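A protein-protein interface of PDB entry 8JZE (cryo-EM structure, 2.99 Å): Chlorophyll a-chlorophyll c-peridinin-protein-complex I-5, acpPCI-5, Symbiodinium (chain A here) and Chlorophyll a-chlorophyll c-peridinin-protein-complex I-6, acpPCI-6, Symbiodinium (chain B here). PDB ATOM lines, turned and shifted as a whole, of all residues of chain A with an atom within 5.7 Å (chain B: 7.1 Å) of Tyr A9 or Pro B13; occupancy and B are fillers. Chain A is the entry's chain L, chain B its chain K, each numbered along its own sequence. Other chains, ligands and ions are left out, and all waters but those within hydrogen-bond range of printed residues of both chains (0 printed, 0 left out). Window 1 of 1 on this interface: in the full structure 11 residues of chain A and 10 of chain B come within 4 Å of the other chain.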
ATOM      1  N   GLU A   4      10.956  -7.731   1.488  1.00  0.00           N
ATOM      2  CA  GLU A   4      10.837  -6.920   0.247  1.00  0.00           C
ATOM      3  C   GLU A   4      11.815  -7.471  -0.795  1.00  0.00           C
ATOM      4  O   GLU A   4      12.929  -7.867  -0.403  1.00  0.00           O
ATOM      5  CB  GLU A   4      11.123  -5.447   0.542  1.00  0.00           C
ATOM      6  CG  GLU A   4      11.363  -4.615  -0.704  1.00  0.00           C
ATOM      7  CD  GLU A   4      10.287  -4.742  -1.768  1.00  0.00           C
ATOM      8  OE1 GLU A   4       9.095  -4.640  -1.416  1.00  0.00           O
ATOM      9  OE2 GLU A   4      10.643  -4.947  -2.945  1.00  0.00           O
ATOM     10  N   LEU A   5      11.414  -7.475  -2.068  1.00  0.00           N
ATOM     11  CA  LEU A   5      12.283  -8.008  -3.151  1.00  0.00           C
ATOM     12  C   LEU A   5      13.657  -7.335  -3.061  1.00  0.00           C
ATOM     13  O   LEU A   5      14.657  -8.002  -3.375  1.00  0.00           O
ATOM     14  CB  LEU A   5      11.618  -7.727  -4.502  1.00  0.00           C
ATOM     15  CG  LEU A   5      10.514  -8.702  -4.912  1.00  0.00           C
ATOM     16  CD1 LEU A   5      10.248  -9.723  -3.816  1.00  0.00           C
ATOM     17  CD2 LEU A   5       9.237  -7.960  -5.272  1.00  0.00           C
ATOM     18  N   ALA A   6      13.698  -6.073  -2.624  1.00  0.00           N
ATOM     19  CA  ALA A   6      14.978  -5.330  -2.539  1.00  0.00           C
ATOM     20  C   ALA A   6      15.994  -6.142  -1.728  1.00  0.00           C
ATOM     21  O   ALA A   6      17.167  -6.208  -2.148  1.00  0.00           O
ATOM     22  CB  ALA A   6      14.742  -3.972  -1.926  1.00  0.00           C
ATOM     23  N   VAL A   7      15.555  -6.735  -0.614  1.00  0.00           N
ATOM     24  CA  VAL A   7      16.464  -7.553   0.242  1.00  0.00           C
ATOM     25  C   VAL A   7      16.217  -9.035  -0.059  1.00  0.00           C
ATOM     26  O   VAL A   7      17.206  -9.774  -0.222  1.00  0.00           O
ATOM     27  CB  VAL A   7      16.262  -7.237   1.736  1.00  0.00           C
ATOM     28  CG1 VAL A   7      14.808  -6.919   2.054  1.00  0.00           C
ATOM     29  CG2 VAL A   7      16.779  -8.355   2.628  1.00  0.00           C
ATOM     30  N   ALA A   8      14.948  -9.446  -0.127  1.00  0.00           N
ATOM     31  CA  ALA A   8      14.619 -10.834  -0.441  1.00  0.00           C
ATOM     32  C   ALA A   8      15.437 -11.353  -1.615  1.00  0.00           C
ATOM     33  O   ALA A   8      15.791 -12.536  -1.658  1.00  0.00           O
ATOM     34  CB  ALA A   8      13.127 -10.970  -0.740  1.00  0.00           C
ATOM     35  N   TYR A   9      15.743 -10.486  -2.582  1.00  0.00           N
ATOM     36  CA  TYR A   9      16.491 -10.918  -3.757  1.00  0.00           C
ATOM     37  C   TYR A   9      17.916 -11.334  -3.421  1.00  0.00           C
ATOM     38  O   TYR A   9      18.567 -11.987  -4.244  1.00  0.00           O
ATOM     39  CB  TYR A   9      16.510  -9.809  -4.811  1.00  0.00           C
ATOM     40  CG  TYR A   9      15.239  -9.712  -5.624  1.00  0.00           C
ATOM     41  CD1 TYR A   9      14.225 -10.649  -5.476  1.00  0.00           C
ATOM     42  CD2 TYR A   9      15.059  -8.692  -6.546  1.00  0.00           C
ATOM     43  CE1 TYR A   9      13.067 -10.566  -6.216  1.00  0.00           C
ATOM     44  CE2 TYR A   9      13.906  -8.602  -7.293  1.00  0.00           C
ATOM     45  CZ  TYR A   9      12.912  -9.544  -7.123  1.00  0.00           C
ATOM     46  OH  TYR A   9      11.756  -9.463  -7.863  1.00  0.00           O
ATOM     47  N   GLU A  10      18.415 -10.979  -2.236  1.00  0.00           N
ATOM     48  CA  GLU A  10      19.771 -11.355  -1.856  1.00  0.00           C
ATOM     49  C   GLU A  10      19.907 -12.838  -1.532  1.00  0.00           C
ATOM     50  O   GLU A  10      21.036 -13.326  -1.427  1.00  0.00           O
ATOM     51  CB  GLU A  10      20.236 -10.516  -0.665  1.00  0.00           C
ATOM     52  CG  GLU A  10      20.418  -9.039  -0.986  1.00  0.00           C
ATOM     53  CD  GLU A  10      21.103  -8.275   0.129  1.00  0.00           C
ATOM     54  OE1 GLU A  10      20.914  -8.640   1.309  1.00  0.00           O
ATOM     55  OE2 GLU A  10      21.837  -7.312  -0.173  1.00  0.00           O
ATOM     56  N   ASP A  11      18.797 -13.558  -1.371  1.00  0.00           N
ATOM     57  CA  ASP A  11      18.818 -14.997  -1.137  1.00  0.00           C
ATOM     58  C   ASP A  11      18.141 -15.757  -2.275  1.00  0.00           C
ATOM     59  O   ASP A  11      17.607 -16.849  -2.069  1.00  0.00           O
ATOM     60  CB  ASP A  11      18.162 -15.344   0.199  1.00  0.00           C
ATOM     61  CG  ASP A  11      18.999 -14.919   1.391  1.00  0.00           C
ATOM     62  OD1 ASP A  11      19.952 -14.135   1.204  1.00  0.00           O
ATOM     63  OD2 ASP A  11      18.707 -15.379   2.515  1.00  0.00           O
ATOM     64  N   ALA A  12      18.156 -15.192  -3.476  1.00  0.00           N
ATOM     65  CA  ALA A  12      17.542 -15.808  -4.642  1.00  0.00           C
ATOM     66  C   ALA A  12      18.562 -16.652  -5.402  1.00  0.00           C
ATOM     67  O   ALA A  12      19.771 -16.572  -5.177  1.00  0.00           O
ATOM     68  CB  ALA A  12      16.935 -14.741  -5.557  1.00  0.00           C
ATOM     69  N   LYS A 123      12.616 -12.028 -13.768  1.00  0.00           N
ATOM     70  CA  LYS A 123      12.183 -12.368 -12.418  1.00  0.00           C
ATOM     71  C   LYS A 123      11.801 -13.837 -12.296  1.00  0.00           C
ATOM     72  O   LYS A 123      11.922 -14.416 -11.211  1.00  0.00           O
ATOM     73  CB  LYS A 123      11.011 -11.471 -12.006  1.00  0.00           C
ATOM     74  CG  LYS A 123       9.848 -12.187 -11.333  1.00  0.00           C
ATOM     75  CD  LYS A 123       9.556 -11.625  -9.949  1.00  0.00           C
ATOM     76  CE  LYS A 123       9.964 -12.606  -8.865  1.00  0.00           C
ATOM     77  NZ  LYS A 123       9.301 -13.928  -9.049  1.00  0.00           N
ATOM     78  N   TRP A 127      16.331 -14.108  -9.762  1.00  0.00           N
ATOM     79  CA  TRP A 127      15.591 -13.412  -8.711  1.00  0.00           C
ATOM     80  C   TRP A 127      14.385 -14.203  -8.212  1.00  0.00           C
ATOM     81  O   TRP A 127      13.608 -13.700  -7.396  1.00  0.00           O
ATOM     82  CB  TRP A 127      15.140 -12.031  -9.197  1.00  0.00           C
ATOM     83  CG  TRP A 127      16.237 -11.247  -9.835  1.00  0.00           C
ATOM     84  CD1 TRP A 127      16.281 -10.787 -11.118  1.00  0.00           C
ATOM     85  CD2 TRP A 127      17.467 -10.850  -9.222  1.00  0.00           C
ATOM     86  NE1 TRP A 127      17.461 -10.118 -11.339  1.00  0.00           N
ATOM     87  CE2 TRP A 127      18.207 -10.145 -10.189  1.00  0.00           C
ATOM     88  CE3 TRP A 127      18.012 -11.018  -7.947  1.00  0.00           C
ATOM     89  CZ2 TRP A 127      19.465  -9.611  -9.921  1.00  0.00           C
ATOM     90  CZ3 TRP A 127      19.259 -10.487  -7.683  1.00  0.00           C
ATOM     91  CH2 TRP A 127      19.971  -9.790  -8.664  1.00  0.00           C
ATOM     92  N   ASN A 128      14.219 -15.435  -8.683  1.00  0.00           N
ATOM     93  CA  ASN A 128      13.114 -16.286  -8.268  1.00  0.00           C
ATOM     94  C   ASN A 128      13.627 -17.298  -7.252  1.00  0.00           C
ATOM     95  O   ASN A 128      14.464 -18.146  -7.582  1.00  0.00           O
ATOM     96  CB  ASN A 128      12.489 -16.998  -9.467  1.00  0.00           C
ATOM     97  CG  ASN A 128      11.093 -17.509  -9.181  1.00  0.00           C
ATOM     98  OD1 ASN A 128      10.409 -17.013  -8.287  1.00  0.00           O
ATOM     99  ND2 ASN A 128      10.661 -18.504  -9.944  1.00  0.00           N
ATOM    100  N   THR A 132      10.324 -15.531  -2.916  1.00  0.00           N
ATOM    101  CA  THR A 132       9.768 -14.491  -3.773  1.00  0.00           C
ATOM    102  C   THR A 132       9.196 -15.071  -5.063  1.00  0.00           C
ATOM    103  O   THR A 132       9.315 -14.477  -6.137  1.00  0.00           O
ATOM    104  CB  THR A 132      10.820 -13.429  -4.087  1.00  0.00           C
ATOM    105  OG1 THR A 132      10.339 -12.568  -5.126  1.00  0.00           O
ATOM    106  CG2 THR A 132      12.116 -14.076  -4.536  1.00  0.00           C
ATOM    107  N   ASP A 135       5.862 -13.197  -6.426  1.00  0.00           N
ATOM    108  CA  ASP A 135       5.786 -11.876  -5.814  1.00  0.00           C
ATOM    109  C   ASP A 135       6.311 -10.846  -6.806  1.00  0.00           C
ATOM    110  O   ASP A 135       7.512 -10.802  -7.093  1.00  0.00           O
ATOM    111  CB  ASP A 135       6.585 -11.850  -4.512  1.00  0.00           C
ATOM    112  CG  ASP A 135       6.324 -10.604  -3.683  1.00  0.00           C
ATOM    113  OD1 ASP A 135       5.894  -9.576  -4.246  1.00  0.00           O
ATOM    114  OD2 ASP A 135       6.562 -10.651  -2.458  1.00  0.00           O
ATOM    115  N   TYR B   3      19.317  -4.380  -2.710  1.00  0.00           N
ATOM    116  CA  TYR B   3      19.694  -3.972  -4.055  1.00  0.00           C
ATOM    117  C   TYR B   3      19.187  -2.567  -4.354  1.00  0.00           C
ATOM    118  O   TYR B   3      18.163  -2.125  -3.826  1.00  0.00           O
ATOM    119  CB  TYR B   3      19.138  -4.954  -5.088  1.00  0.00           C
ATOM    120  CG  TYR B   3      19.953  -6.216  -5.258  1.00  0.00           C
ATOM    121  CD1 TYR B   3      20.971  -6.282  -6.200  1.00  0.00           C
ATOM    122  CD2 TYR B   3      19.696  -7.344  -4.489  1.00  0.00           C
ATOM    123  CE1 TYR B   3      21.714  -7.431  -6.366  1.00  0.00           C
ATOM    124  CE2 TYR B   3      20.434  -8.498  -4.648  1.00  0.00           C
ATOM    125  CZ  TYR B   3      21.443  -8.535  -5.588  1.00  0.00           C
ATOM    126  OH  TYR B   3      22.183  -9.682  -5.750  1.00  0.00           O
ATOM    127  N   LYS B   4      19.921  -1.859  -5.210  1.00  0.00           N
ATOM    128  CA  LYS B   4      19.450  -0.576  -5.713  1.00  0.00           C
ATOM    129  C   LYS B   4      18.310  -0.843  -6.684  1.00  0.00           C
ATOM    130  O   LYS B   4      18.536  -1.060  -7.879  1.00  0.00           O
ATOM    131  CB  LYS B   4      20.584   0.201  -6.389  1.00  0.00           C
ATOM    132  CG  LYS B   4      20.182   1.563  -6.936  1.00  0.00           C
ATOM    133  CD  LYS B   4      19.694   2.484  -5.833  1.00  0.00           C
ATOM    134  CE  LYS B   4      19.356   3.863  -6.376  1.00  0.00           C
ATOM    135  NZ  LYS B   4      18.335   3.805  -7.459  1.00  0.00           N
ATOM    136  N   MET B   5      17.084  -0.843  -6.174  1.00  0.00           N
ATOM    137  CA  MET B   5      15.940  -1.267  -6.967  1.00  0.00           C
ATOM    138  C   MET B   5      15.628  -0.249  -8.057  1.00  0.00           C
ATOM    139  O   MET B   5      15.653   0.962  -7.826  1.00  0.00           O
ATOM    140  CB  MET B   5      14.727  -1.470  -6.064  1.00  0.00           C
ATOM    141  CG  MET B   5      13.629  -2.307  -6.680  1.00  0.00           C
ATOM    142  SD  MET B   5      14.186  -3.941  -7.201  1.00  0.00           S
ATOM    143  CE  MET B   5      14.978  -4.535  -5.712  1.00  0.00           C
ATOM    144  N   SER B   6      15.336  -0.752  -9.254  1.00  0.00           N
ATOM    145  CA  SER B   6      14.993   0.123 -10.365  1.00  0.00           C
ATOM    146  C   SER B   6      13.676   0.833 -10.087  1.00  0.00           C
ATOM    147  O   SER B   6      12.735   0.245  -9.549  1.00  0.00           O
ATOM    148  CB  SER B   6      14.892  -0.671 -11.667  1.00  0.00           C
ATOM    149  OG  SER B   6      13.706  -1.444 -11.697  1.00  0.00           O
ATOM    150  N   LYS B   7      13.619   2.114 -10.449  1.00  0.00           N
ATOM    151  CA  LYS B   7      12.410   2.891 -10.210  1.00  0.00           C
ATOM    152  C   LYS B   7      11.306   2.525 -11.192  1.00  0.00           C
ATOM    153  O   LYS B   7      10.128   2.489 -10.819  1.00  0.00           O
ATOM    154  CB  LYS B   7      12.724   4.385 -10.284  1.00  0.00           C
ATOM    155  CG  LYS B   7      13.738   4.843  -9.246  1.00  0.00           C
ATOM    156  CD  LYS B   7      13.891   6.355  -9.239  1.00  0.00           C
ATOM    157  CE  LYS B   7      14.923   6.797  -8.214  1.00  0.00           C
ATOM    158  NZ  LYS B   7      15.134   8.271  -8.232  1.00  0.00           N
ATOM    159  N   VAL B   9      10.774  -0.506 -13.128  1.00  0.00           N
ATOM    160  CA  VAL B   9      10.251  -1.842 -12.852  1.00  0.00           C
ATOM    161  C   VAL B   9      10.552  -2.181 -11.396  1.00  0.00           C
ATOM    162  O   VAL B   9      11.661  -2.638 -11.084  1.00  0.00           O
ATOM    163  CB  VAL B   9      10.848  -2.882 -13.811  1.00  0.00           C
ATOM    164  CG1 VAL B   9      10.199  -4.229 -13.596  1.00  0.00           C
ATOM    165  CG2 VAL B   9      10.667  -2.431 -15.248  1.00  0.00           C
ATOM    166  N   PRO B  10       9.602  -1.975 -10.479  1.00  0.00           N
ATOM    167  CA  PRO B  10       9.929  -2.071  -9.046  1.00  0.00           C
ATOM    168  C   PRO B  10      10.322  -3.460  -8.583  1.00  0.00           C
ATOM    169  O   PRO B  10      10.934  -3.583  -7.516  1.00  0.00           O
ATOM    170  CB  PRO B  10       8.636  -1.604  -8.358  1.00  0.00           C
ATOM    171  CG  PRO B  10       7.851  -0.903  -9.422  1.00  0.00           C
ATOM    172  CD  PRO B  10       8.192  -1.615 -10.689  1.00  0.00           C
ATOM    173  N   PHE B  11       9.984  -4.509  -9.326  1.00  0.00           N
ATOM    174  CA  PHE B  11      10.315  -5.866  -8.915  1.00  0.00           C
ATOM    175  C   PHE B  11      11.606  -6.379  -9.539  1.00  0.00           C
ATOM    176  O   PHE B  11      11.928  -7.559  -9.379  1.00  0.00           O
ATOM    177  CB  PHE B  11       9.158  -6.820  -9.235  1.00  0.00           C
ATOM    178  CG  PHE B  11       8.677  -6.755 -10.655  1.00  0.00           C
ATOM    179  CD1 PHE B  11       7.649  -5.900 -11.012  1.00  0.00           C
ATOM    180  CD2 PHE B  11       9.232  -7.571 -11.626  1.00  0.00           C
ATOM    181  CE1 PHE B  11       7.197  -5.845 -12.313  1.00  0.00           C
ATOM    182  CE2 PHE B  11       8.784  -7.522 -12.929  1.00  0.00           C
ATOM    183  CZ  PHE B  11       7.763  -6.659 -13.273  1.00  0.00           C
ATOM    184  N   LEU B  12      12.352  -5.523 -10.238  1.00  0.00           N
ATOM    185  CA  LEU B  12      13.622  -5.904 -10.837  1.00  0.00           C
ATOM    186  C   LEU B  12      14.696  -4.915 -10.397  1.00  0.00           C
ATOM    187  O   LEU B  12      14.500  -3.693 -10.518  1.00  0.00           O
ATOM    188  CB  LEU B  12      13.525  -5.942 -12.369  1.00  0.00           C
ATOM    189  CG  LEU B  12      13.612  -7.322 -13.023  1.00  0.00           C
ATOM    190  CD1 LEU B  12      12.583  -8.256 -12.431  1.00  0.00           C
ATOM    191  CD2 LEU B  12      13.424  -7.220 -14.523  1.00  0.00           C
ATOM    192  N   PRO B  13      15.825  -5.389  -9.874  1.00  0.00           N
ATOM    193  CA  PRO B  13      16.894  -4.468  -9.475  1.00  0.00           C
ATOM    194  C   PRO B  13      17.480  -3.742 -10.675  1.00  0.00           C
ATOM    195  O   PRO B  13      17.538  -4.270 -11.786  1.00  0.00           O
ATOM    196  CB  PRO B  13      17.930  -5.388  -8.820  1.00  0.00           C
ATOM    197  CG  PRO B  13      17.680  -6.720  -9.430  1.00  0.00           C
ATOM    198  CD  PRO B  13      16.200  -6.796  -9.658  1.00  0.00           C
ATOM    199  N   MET B  14      17.919  -2.509 -10.433  1.00  0.00           N
ATOM    200  CA  MET B  14      18.466  -1.690 -11.506  1.00  0.00           C
ATOM    201  C   MET B  14      19.821  -2.227 -11.949  1.00  0.00           C
ATOM    202  O   MET B  14      20.659  -2.604 -11.125  1.00  0.00           O
ATOM    203  CB  MET B  14      18.594  -0.235 -11.054  1.00  0.00           C
ATOM    204  CG  MET B  14      18.545   0.772 -12.194  1.00  0.00           C
ATOM    205  SD  MET B  14      18.764   2.474 -11.645  1.00  0.00           S
ATOM    206  CE  MET B  14      20.461   2.423 -11.085  1.00  0.00           C
ATOM    207  N   SER B  15      20.032  -2.265 -13.262  1.00  0.00           N
ATOM    208  CA  SER B  15      21.291  -2.761 -13.795  1.00  0.00           C
ATOM    209  C   SER B  15      22.429  -1.813 -13.422  1.00  0.00           C
ATOM    210  O   SER B  15      22.264  -0.590 -13.476  1.00  0.00           O
ATOM    211  CB  SER B  15      21.212  -2.913 -15.312  1.00  0.00           C
ATOM    212  OG  SER B  15      20.852  -1.690 -15.924  1.00  0.00           O
ATOM    213  N   PRO B  16      23.589  -2.346 -13.034  1.00  0.00           N
ATOM    214  CA  PRO B  16      24.693  -1.472 -12.607  1.00  0.00           C
ATOM    215  C   PRO B  16      25.206  -0.551 -13.698  1.00  0.00           C
ATOM    216  O   PRO B  16      25.821   0.474 -13.380  1.00  0.00           O
ATOM    217  CB  PRO B  16      25.774  -2.466 -12.160  1.00  0.00           C
ATOM    218  CG  PRO B  16      25.035  -3.731 -11.865  1.00  0.00           C
ATOM    219  CD  PRO B  16      23.908  -3.771 -12.849  1.00  0.00           C
ATOM    220  N   GLY B  28      15.698   4.136 -14.532  1.00  0.00           N
ATOM    221  CA  GLY B  28      16.386   2.853 -14.536  1.00  0.00           C
ATOM    222  C   GLY B  28      15.638   1.746 -15.243  1.00  0.00           C
ATOM    223  O   GLY B  28      15.644   0.601 -14.774  1.00  0.00           O
ATOM    224  N   ASP B  30      15.231  -1.070 -17.498  1.00  0.00           N
ATOM    225  CA  ASP B  30      15.902  -2.091 -18.289  1.00  0.00           C
ATOM    226  C   ASP B  30      15.501  -3.471 -17.781  1.00  0.00           C
ATOM    227  O   ASP B  30      16.332  -4.188 -17.208  1.00  0.00           O
ATOM    228  CB  ASP B  30      17.420  -1.926 -18.232  1.00  0.00           C
ATOM    229  CG  ASP B  30      18.135  -2.796 -19.243  1.00  0.00           C
ATOM    230  OD1 ASP B  30      17.472  -3.289 -20.180  1.00  0.00           O
ATOM    231  OD2 ASP B  30      19.357  -2.992 -19.099  1.00  0.00           O
ATOM    232  N   PRO B  31      14.243  -3.878 -17.971  1.00  0.00           N
ATOM    233  CA  PRO B  31      13.821  -5.184 -17.450  1.00  0.00           C
ATOM    234  C   PRO B  31      14.449  -6.355 -18.179  1.00  0.00           C
ATOM    235  O   PRO B  31      14.748  -7.373 -17.544  1.00  0.00           O
ATOM    236  CB  PRO B  31      12.299  -5.157 -17.631  1.00  0.00           C
ATOM    237  CG  PRO B  31      12.084  -4.242 -18.777  1.00  0.00           C
ATOM    238  CD  PRO B  31      13.157  -3.194 -18.692  1.00  0.00           C
ATOM    239  N   LEU B  36      22.997  -5.199 -19.482  1.00  0.00           N
ATOM    240  CA  LEU B  36      23.795  -6.261 -18.888  1.00  0.00           C
ATOM    241  C   LEU B  36      24.530  -7.095 -19.928  1.00  0.00           C
ATOM    242  O   LEU B  36      25.422  -7.865 -19.560  1.00  0.00           O
ATOM    243  CB  LEU B  36      22.903  -7.174 -18.039  1.00  0.00           C
ATOM    244  CG  LEU B  36      22.184  -6.530 -16.851  1.00  0.00           C
ATOM    245  CD1 LEU B  36      21.184  -7.491 -16.235  1.00  0.00           C
ATOM    246  CD2 LEU B  36      23.181  -6.069 -15.808  1.00  0.00           C
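CA of Ala A6 touches CE of Met B5, at 3.3 Å.
Tyr B3 touches Tyr A9.
Pro B13 touches Tyr A9 (CD to CE2, 3.8 Å).
Glu A10 touches Tyr B3 (CG to CE2, 3.7 Å).
Lys A123 touches Leu B12 (CB to CD1, 3.6 Å).
Tyr B3 touches Trp A127 (OH to CZ3, 3.6 Å).
Pro B13 touches Trp A127.
Of the 14 printed residues of chain A, 5 touch a printed residue of chain B.
Printed residues of chain A that touch a printed residue of chain B: Ala A6, Tyr A9, Glu A10, Lys A123 and Trp A127.
Hydrophobic or aromatic side chains of chain A that line the printed part of chain B: Ala A6, Tyr A9 and Trp A127.
Of the 17 printed residues of chain B, 5 touch a printed residue of chain A.
Hydrophobic or aromatic side chains of chain B that line the printed part of chain A: Tyr B3, Met B5, Phe B11, Leu B12 and Pro B13.
The side-chain hydroxyl (OG) of Ser B6 sits at hydrogen-bond distance from the backbone carbonyl oxygen (O) of Leu B12 (2.7 Å).
OE2 of Glu A4 lies close to N of Ala A6 (3.3 Å).
NZ of Lys A123 is in hydrogen-bond range of OD1 of Asn A128, at 3.4 Å.
The side-chain amino group of Lys A123 is in hydrogen-bond range of the backbone carbonyl oxygen of Thr A132 (3.0 Å).
The backbone carbonyl oxygen (O) of Ala A6 sits at hydrogen-bond distance from the backbone NH (N) of Tyr B3 (2.9 Å).
The backbone carbonyl oxygen (O) of Phe B11 lies within hydrogen-bond range of the side-chain hydroxyl (OH) of Tyr A9, 2.4 Å away.
Of the printed residues of chain B, Tyr A9 touches Tyr B3 (3.98 Å), Phe B11 (2.4 Å) and Pro B13 (3.8 Å).
Printed residues of chain B within 4 Å of Glu A10: Tyr B3 (3.7 Å).
Of the printed residues of chain B, Trp A127 touches Tyr B3 and Pro B13.
Of the printed residues of chain A, Tyr B3 touches Ala A6, Tyr A9, Glu A10 and Trp A127.
Of the printed residues of chain A, Leu B12 touches Lys A123.
Pro B13 touches just these residues of chain A: Tyr A9 and Trp A127.
Met B14 touches none of the printed residues of chain A.
The nearest residue of chain B that does not touch Tyr A9 is Met B5 (4.2 Å).
The nearest printed residue of chain A that does not touch Pro B13 is Leu A5 (6.6 Å).
The nearest printed residue of chain A that does not touch Met B5 is Leu A5 (4.1 Å).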
